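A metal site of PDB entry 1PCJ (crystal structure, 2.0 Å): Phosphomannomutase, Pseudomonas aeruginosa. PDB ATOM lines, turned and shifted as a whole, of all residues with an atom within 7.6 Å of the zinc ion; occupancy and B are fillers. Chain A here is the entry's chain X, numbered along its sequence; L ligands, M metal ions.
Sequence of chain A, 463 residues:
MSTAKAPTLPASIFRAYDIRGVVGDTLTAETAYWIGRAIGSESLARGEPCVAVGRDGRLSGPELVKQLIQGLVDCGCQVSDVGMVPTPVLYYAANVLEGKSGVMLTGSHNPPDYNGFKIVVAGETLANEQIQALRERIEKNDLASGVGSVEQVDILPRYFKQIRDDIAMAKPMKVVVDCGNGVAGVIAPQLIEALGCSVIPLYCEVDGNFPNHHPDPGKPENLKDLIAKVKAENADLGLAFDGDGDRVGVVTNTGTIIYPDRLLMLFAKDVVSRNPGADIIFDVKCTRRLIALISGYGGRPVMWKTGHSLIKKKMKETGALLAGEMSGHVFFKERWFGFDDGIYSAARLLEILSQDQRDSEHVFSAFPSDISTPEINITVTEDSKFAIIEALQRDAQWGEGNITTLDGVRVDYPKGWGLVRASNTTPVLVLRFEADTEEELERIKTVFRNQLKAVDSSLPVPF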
ATOM      1  N   ARG A  20     -27.154   3.615  -2.199  1.00  0.00           N
ATOM      2  CA  ARG A  20     -25.926   3.295  -2.961  1.00  0.00           C
ATOM      3  C   ARG A  20     -24.727   3.804  -2.156  1.00  0.00           C
ATOM      4  O   ARG A  20     -24.704   4.972  -1.733  1.00  0.00           O
ATOM      5  CB  ARG A  20     -25.930   3.975  -4.348  1.00  0.00           C
ATOM      6  CG  ARG A  20     -26.891   3.373  -5.409  1.00  0.00           C
ATOM      7  CD  ARG A  20     -26.999   4.174  -6.753  1.00  0.00           C
ATOM      8  NE  ARG A  20     -28.229   3.803  -7.479  1.00  0.00           N
ATOM      9  CZ  ARG A  20     -28.291   3.115  -8.648  1.00  0.00           C
ATOM     10  NH1 ARG A  20     -27.202   2.758  -9.315  1.00  0.00           N
ATOM     11  NH2 ARG A  20     -29.491   2.820  -9.166  1.00  0.00           N
ATOM     12  N   THR A  87     -31.091  -8.955  -9.887  1.00  0.00           N
ATOM     13  CA  THR A  87     -32.096  -8.027  -9.397  1.00  0.00           C
ATOM     14  C   THR A  87     -33.546  -8.363  -9.790  1.00  0.00           C
ATOM     15  O   THR A  87     -34.414  -8.444  -8.920  1.00  0.00           O
ATOM     16  CB  THR A  87     -31.698  -6.605  -9.821  1.00  0.00           C
ATOM     17  OG1 THR A  87     -30.571  -6.187  -9.027  1.00  0.00           O
ATOM     18  CG2 THR A  87     -32.800  -5.606  -9.517  1.00  0.00           C
ATOM     19  N   PRO A  88     -33.843  -8.532 -11.082  1.00  0.00           N
ATOM     20  CA  PRO A  88     -35.195  -8.909 -11.474  1.00  0.00           C
ATOM     21  C   PRO A  88     -35.713 -10.223 -10.886  1.00  0.00           C
ATOM     22  O   PRO A  88     -36.932 -10.348 -10.763  1.00  0.00           O
ATOM     23  CB  PRO A  88     -35.104  -9.012 -13.004  1.00  0.00           C
ATOM     24  CG  PRO A  88     -33.667  -9.156 -13.287  1.00  0.00           C
ATOM     25  CD  PRO A  88     -32.978  -8.316 -12.258  1.00  0.00           C
ATOM     26  N   THR A 106     -27.345  -4.834  -3.996  1.00  0.00           N
ATOM     27  CA  THR A 106     -26.607  -4.706  -5.233  1.00  0.00           C
ATOM     28  C   THR A 106     -25.950  -3.331  -5.414  1.00  0.00           C
ATOM     29  O   THR A 106     -26.492  -2.314  -4.973  1.00  0.00           O
ATOM     30  CB  THR A 106     -27.538  -5.032  -6.425  1.00  0.00           C
ATOM     31  OG1 THR A 106     -26.797  -5.018  -7.648  1.00  0.00           O
ATOM     32  CG2 THR A 106     -28.638  -3.966  -6.619  1.00  0.00           C
ATOM     33  N   GLY A 107     -24.792  -3.337  -6.061  1.00  0.00           N
ATOM     34  CA  GLY A 107     -24.121  -2.131  -6.536  1.00  0.00           C
ATOM     35  C   GLY A 107     -24.253  -1.917  -8.042  1.00  0.00           C
ATOM     36  O   GLY A 107     -23.464  -1.192  -8.641  1.00  0.00           O
ATOM     37  N   SEP A 108     -25.248  -2.573  -8.652  1.00  0.00           N
ATOM     38  CA  SEP A 108     -25.629  -2.397 -10.055  1.00  0.00           C
ATOM     39  CB  SEP A 108     -26.387  -1.069 -10.245  1.00  0.00           C
ATOM     40  OG  SEP A 108     -26.837  -0.958 -11.591  1.00  0.00           O
ATOM     41  C   SEP A 108     -24.448  -2.575 -11.034  1.00  0.00           C
ATOM     42  O   SEP A 108     -23.897  -3.665 -11.133  1.00  0.00           O
ATOM     43  P   SEP A 108     -28.101   0.013 -11.886  1.00  0.00           P
ATOM     44  O1P SEP A 108     -27.492   1.376 -12.433  1.00  0.00           O
ATOM     45  O2P SEP A 108     -28.956   0.279 -10.543  1.00  0.00           O
ATOM     46  O3P SEP A 108     -29.005  -0.672 -12.997  1.00  0.00           O
ATOM     47  N   HIS A 109     -24.050  -1.500 -11.725  1.00  0.00           N
ATOM     48  CA  HIS A 109     -23.001  -1.552 -12.761  1.00  0.00           C
ATOM     49  C   HIS A 109     -21.681  -0.951 -12.272  1.00  0.00           C
ATOM     50  O   HIS A 109     -20.703  -0.878 -13.024  1.00  0.00           O
ATOM     51  CB  HIS A 109     -23.474  -0.769 -13.990  1.00  0.00           C
ATOM     52  CG  HIS A 109     -23.549   0.718 -13.766  1.00  0.00           C
ATOM     53  ND1 HIS A 109     -24.643   1.340 -13.202  1.00  0.00           N
ATOM     54  CD2 HIS A 109     -22.644   1.704 -14.024  1.00  0.00           C
ATOM     55  CE1 HIS A 109     -24.417   2.646 -13.118  1.00  0.00           C
ATOM     56  NE2 HIS A 109     -23.219   2.893 -13.615  1.00  0.00           N
ATOM     57  N   ASN A 110     -21.659  -0.487 -11.019  1.00  0.00           N
ATOM     58  CA  ASN A 110     -20.516   0.272 -10.483  1.00  0.00           C
ATOM     59  C   ASN A 110     -19.295  -0.598 -10.183  1.00  0.00           C
ATOM     60  O   ASN A 110     -19.403  -1.827 -10.190  1.00  0.00           O
ATOM     61  CB  ASN A 110     -20.952   1.038  -9.237  1.00  0.00           C
ATOM     62  CG  ASN A 110     -21.977   2.117  -9.540  1.00  0.00           C
ATOM     63  OD1 ASN A 110     -23.009   2.213  -8.878  1.00  0.00           O
ATOM     64  ND2 ASN A 110     -21.678   2.961 -10.522  1.00  0.00           N
ATOM     65  N   LYS A 118     -31.887  -1.941  -3.329  1.00  0.00           N
ATOM     66  CA  LYS A 118     -33.106  -1.582  -4.034  1.00  0.00           C
ATOM     67  C   LYS A 118     -34.250  -2.229  -3.275  1.00  0.00           C
ATOM     68  O   LYS A 118     -34.190  -3.435  -2.940  1.00  0.00           O
ATOM     69  CB  LYS A 118     -33.029  -2.042  -5.491  1.00  0.00           C
ATOM     70  CG  LYS A 118     -31.789  -1.517  -6.190  1.00  0.00           C
ATOM     71  CD  LYS A 118     -31.658  -2.041  -7.602  1.00  0.00           C
ATOM     72  CE  LYS A 118     -30.707  -1.217  -8.402  1.00  0.00           C
ATOM     73  NZ  LYS A 118     -30.554  -1.763  -9.770  1.00  0.00           N
ATOM     74  N   PRO A 215     -19.397  -4.400 -16.054  1.00  0.00           N
ATOM     75  CA  PRO A 215     -20.687  -4.801 -16.628  1.00  0.00           C
ATOM     76  C   PRO A 215     -21.632  -3.606 -16.731  1.00  0.00           C
ATOM     77  O   PRO A 215     -22.533  -3.410 -15.914  1.00  0.00           O
ATOM     78  CB  PRO A 215     -21.188  -5.861 -15.638  1.00  0.00           C
ATOM     79  CG  PRO A 215     -20.589  -5.459 -14.329  1.00  0.00           C
ATOM     80  CD  PRO A 215     -19.271  -4.804 -14.643  1.00  0.00           C
ATOM     81  N   PRO A 217     -23.357  -1.965 -20.028  1.00  0.00           N
ATOM     82  CA  PRO A 217     -23.577  -1.981 -21.484  1.00  0.00           C
ATOM     83  C   PRO A 217     -24.021  -0.641 -22.078  1.00  0.00           C
ATOM     84  O   PRO A 217     -24.222  -0.565 -23.293  1.00  0.00           O
ATOM     85  CB  PRO A 217     -24.677  -3.029 -21.646  1.00  0.00           C
ATOM     86  CG  PRO A 217     -25.444  -2.984 -20.387  1.00  0.00           C
ATOM     87  CD  PRO A 217     -24.462  -2.611 -19.306  1.00  0.00           C
ATOM     88  N   PHE A 241     -25.505  -7.800 -20.580  1.00  0.00           N
ATOM     89  CA  PHE A 241     -26.206  -7.435 -19.357  1.00  0.00           C
ATOM     90  C   PHE A 241     -25.309  -6.628 -18.437  1.00  0.00           C
ATOM     91  O   PHE A 241     -24.071  -6.751 -18.478  1.00  0.00           O
ATOM     92  CB  PHE A 241     -26.689  -8.688 -18.668  1.00  0.00           C
ATOM     93  CG  PHE A 241     -27.590  -9.505 -19.517  1.00  0.00           C
ATOM     94  CD1 PHE A 241     -28.904  -9.108 -19.712  1.00  0.00           C
ATOM     95  CD2 PHE A 241     -27.118 -10.641 -20.150  1.00  0.00           C
ATOM     96  CE1 PHE A 241     -29.738  -9.855 -20.518  1.00  0.00           C
ATOM     97  CE2 PHE A 241     -27.951 -11.388 -20.956  1.00  0.00           C
ATOM     98  CZ  PHE A 241     -29.268 -10.995 -21.138  1.00  0.00           C
ATOM     99  N   ASP A 242     -25.923  -5.756 -17.648  1.00  0.00           N
ATOM    100  CA  ASP A 242     -25.202  -5.027 -16.630  1.00  0.00           C
ATOM    101  C   ASP A 242     -25.000  -5.937 -15.419  1.00  0.00           C
ATOM    102  O   ASP A 242     -25.452  -7.094 -15.425  1.00  0.00           O
ATOM    103  CB  ASP A 242     -25.879  -3.678 -16.300  1.00  0.00           C
ATOM    104  CG  ASP A 242     -27.028  -3.776 -15.291  1.00  0.00           C
ATOM    105  OD1 ASP A 242     -27.725  -4.817 -15.246  1.00  0.00           O
ATOM    106  OD2 ASP A 242     -27.325  -2.828 -14.519  1.00  0.00           O
ATOM    107  N   GLY A 243     -24.318  -5.440 -14.402  1.00  0.00           N
ATOM    108  CA  GLY A 243     -23.897  -6.271 -13.273  1.00  0.00           C
ATOM    109  C   GLY A 243     -25.011  -7.042 -12.574  1.00  0.00           C
ATOM    110  O   GLY A 243     -24.799  -8.178 -12.172  1.00  0.00           O
ATOM    111  N   ASP A 244     -26.180  -6.441 -12.432  1.00  0.00           N
ATOM    112  CA  ASP A 244     -27.263  -7.067 -11.669  1.00  0.00           C
ATOM    113  C   ASP A 244     -28.418  -7.566 -12.537  1.00  0.00           C
ATOM    114  O   ASP A 244     -29.406  -8.101 -12.036  1.00  0.00           O
ATOM    115  CB  ASP A 244     -27.738  -6.145 -10.535  1.00  0.00           C
ATOM    116  CG  ASP A 244     -28.294  -4.813 -11.042  1.00  0.00           C
ATOM    117  OD1 ASP A 244     -29.231  -4.259 -10.436  1.00  0.00           O
ATOM    118  OD2 ASP A 244     -27.817  -4.233 -12.028  1.00  0.00           O
ATOM    119  N   GLY A 245     -28.286  -7.407 -13.853  1.00  0.00           N
ATOM    120  CA  GLY A 245     -29.205  -7.985 -14.816  1.00  0.00           C
ATOM    121  C   GLY A 245     -30.510  -7.251 -15.076  1.00  0.00           C
ATOM    122  O   GLY A 245     -31.390  -7.824 -15.743  1.00  0.00           O
ATOM    123  N   ASP A 246     -30.670  -6.037 -14.557  1.00  0.00           N
ATOM    124  CA  ASP A 246     -31.872  -5.265 -14.845  1.00  0.00           C
ATOM    125  C   ASP A 246     -31.731  -4.327 -16.043  1.00  0.00           C
ATOM    126  O   ASP A 246     -32.684  -3.621 -16.388  1.00  0.00           O
ATOM    127  CB  ASP A 246     -32.355  -4.491 -13.606  1.00  0.00           C
ATOM    128  CG  ASP A 246     -31.337  -3.542 -13.063  1.00  0.00           C
ATOM    129  OD1 ASP A 246     -30.223  -3.412 -13.604  1.00  0.00           O
ATOM    130  OD2 ASP A 246     -31.567  -2.878 -12.037  1.00  0.00           O
ATOM    131  N   ARG A 247     -30.545  -4.305 -16.654  1.00  0.00           N
ATOM    132  CA  ARG A 247     -30.325  -3.587 -17.900  1.00  0.00           C
ATOM    133  C   ARG A 247     -29.792  -4.541 -18.956  1.00  0.00           C
ATOM    134  O   ARG A 247     -29.042  -5.460 -18.648  1.00  0.00           O
ATOM    135  CB  ARG A 247     -29.307  -2.481 -17.716  1.00  0.00           C
ATOM    136  CG  ARG A 247     -29.758  -1.386 -16.790  1.00  0.00           C
ATOM    137  CD  ARG A 247     -29.042  -0.107 -17.017  1.00  0.00           C
ATOM    138  NE  ARG A 247     -27.683  -0.169 -16.511  1.00  0.00           N
ATOM    139  CZ  ARG A 247     -26.655   0.526 -17.010  1.00  0.00           C
ATOM    140  NH1 ARG A 247     -26.803   1.349 -18.047  1.00  0.00           N
ATOM    141  NH2 ARG A 247     -25.468   0.379 -16.460  1.00  0.00           N
ATOM    142  N   VAL A 248     -30.175  -4.276 -20.198  1.00  0.00           N
ATOM    143  CA  VAL A 248     -29.692  -5.027 -21.354  1.00  0.00           C
ATOM    144  C   VAL A 248     -29.184  -4.056 -22.429  1.00  0.00           C
ATOM    145  O   VAL A 248     -29.688  -2.943 -22.576  1.00  0.00           O
ATOM    146  CB  VAL A 248     -30.817  -5.943 -21.903  1.00  0.00           C
ATOM    147  CG1 VAL A 248     -32.014  -5.121 -22.408  1.00  0.00           C
ATOM    148  CG2 VAL A 248     -30.289  -6.854 -23.015  1.00  0.00           C
ATOM    149  N   HIS A 329     -33.054  -0.091 -18.849  1.00  0.00           N
ATOM    150  CA  HIS A 329     -34.056  -0.655 -17.946  1.00  0.00           C
ATOM    151  C   HIS A 329     -35.342  -0.727 -18.747  1.00  0.00           C
ATOM    152  O   HIS A 329     -35.846   0.302 -19.166  1.00  0.00           O
ATOM    153  CB  HIS A 329     -34.318   0.255 -16.720  1.00  0.00           C
ATOM    154  CG  HIS A 329     -33.204   0.292 -15.725  1.00  0.00           C
ATOM    155  ND1 HIS A 329     -32.853  -0.794 -14.955  1.00  0.00           N
ATOM    156  CD2 HIS A 329     -32.393   1.293 -15.344  1.00  0.00           C
ATOM    157  CE1 HIS A 329     -31.838  -0.467 -14.182  1.00  0.00           C
ATOM    158  NE2 HIS A 329     -31.536   0.794 -14.387  1.00  0.00           N
ATOM    159  N   ASP A 340     -38.451  -3.940 -14.093  1.00  0.00           N
ATOM    160  CA  ASP A 340     -37.349  -3.940 -15.065  1.00  0.00           C
ATOM    161  C   ASP A 340     -36.524  -5.219 -14.960  1.00  0.00           C
ATOM    162  O   ASP A 340     -36.218  -5.702 -13.866  1.00  0.00           O
ATOM    163  CB  ASP A 340     -36.428  -2.729 -14.924  1.00  0.00           C
ATOM    164  CG  ASP A 340     -36.096  -2.388 -13.477  1.00  0.00           C
ATOM    165  OD1 ASP A 340     -34.947  -1.939 -13.233  1.00  0.00           O
ATOM    166  OD2 ASP A 340     -36.914  -2.494 -12.529  1.00  0.00           O
HETATM  167  O1  LIG L   1     -29.654   2.578 -13.209  1.00  0.00           O
HETATM  168  C1  LIG L   1     -30.145   3.589 -12.330  1.00  0.00           C
HETATM  169  C2  LIG L   1     -30.354   4.873 -13.125  1.00  0.00           C
HETATM  170  O2  LIG L   1     -29.039   5.453 -13.469  1.00  0.00           O
HETATM  171  C3  LIG L   1     -29.161   6.722 -14.190  1.00  0.00           C
HETATM  172  O3  LIG L   1     -29.848   7.661 -13.396  1.00  0.00           O
HETATM  173  P1  LIG L   1     -29.300   9.170 -13.380  1.00  0.00           P
HETATM  174  O4  LIG L   1     -29.360   9.774 -14.756  1.00  0.00           O
HETATM  175  O5  LIG L   1     -27.874   9.194 -12.880  1.00  0.00           O
HETATM  176  O6  LIG L   1     -30.213   9.932 -12.460  1.00  0.00           O
HETATM  177  C4  LIG L   1     -29.966   6.537 -15.471  1.00  0.00           C
HETATM  178  O7  LIG L   1     -29.184   5.677 -16.357  1.00  0.00           O
HETATM  179  C5  LIG L   1     -31.344   5.878 -15.178  1.00  0.00           C
HETATM  180  O8  LIG L   1     -31.990   5.567 -16.411  1.00  0.00           O
HETATM  181  C6  LIG L   1     -31.176   4.594 -14.370  1.00  0.00           C
HETATM  182  O9  LIG L   1     -32.457   4.091 -13.973  1.00  0.00           O
HETATM  183 ZN    ZN M   1     -28.570  -2.708 -13.067  1.00  0.00          ZN
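O1P of SEP 108 is in hydrogen-bond range of O1 of the ligand, at 2.6 Å. A ring nitrogen (NE2) of His 329 is in hydrogen-bond range of an oxygen (O1) of the ligand, at 2.8 Å.
The side-chain amino group (NZ) of Lys 118 lies within salt-bridge range of the side-chain carboxylate (OD2) of Asp 246, at 2.7 Å. A ring nitrogen (ND1) of His 329 lies within hydrogen-bond range of the backbone carbonyl oxygen of Asp 246, 3.2 Å away. The side-chain carboxylate (OD1) of Asp 242 sits at hydrogen-bond distance from the backbone NH (N) of Gly 245, 3.0 Å away. O2P of SEP 108 lies within salt-bridge range of the side-chain amino group (NZ) of Lys 118 (2.7 Å). O3P of SEP 108 lies close to NE2 of His 329 (3.2 Å). NE of Arg 247 lies close to O3P of SEP 108 (3.8 Å). O1P of SEP 108 sits at hydrogen-bond distance from a ring nitrogen (ND1) of His 109 (3.0 Å). NH2 of Arg 20 lies within salt-bridge range of O2P of SEP 108 (2.9 Å).
Lys 118 touches the zinc ion. Within 4 Å of the zinc ion: SEP 108, Lys 118, Asp 242, Asp 244 and Asp 246.
The zinc ion is bound by the side-chain carboxylate (OD1) of Asp 246, the side-chain carboxylate (OD2) of Asp 242, the side-chain carboxylate (OD2) of Asp 244 and O3P of SEP 108. The zinc ion has four donor atoms within binding distance.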
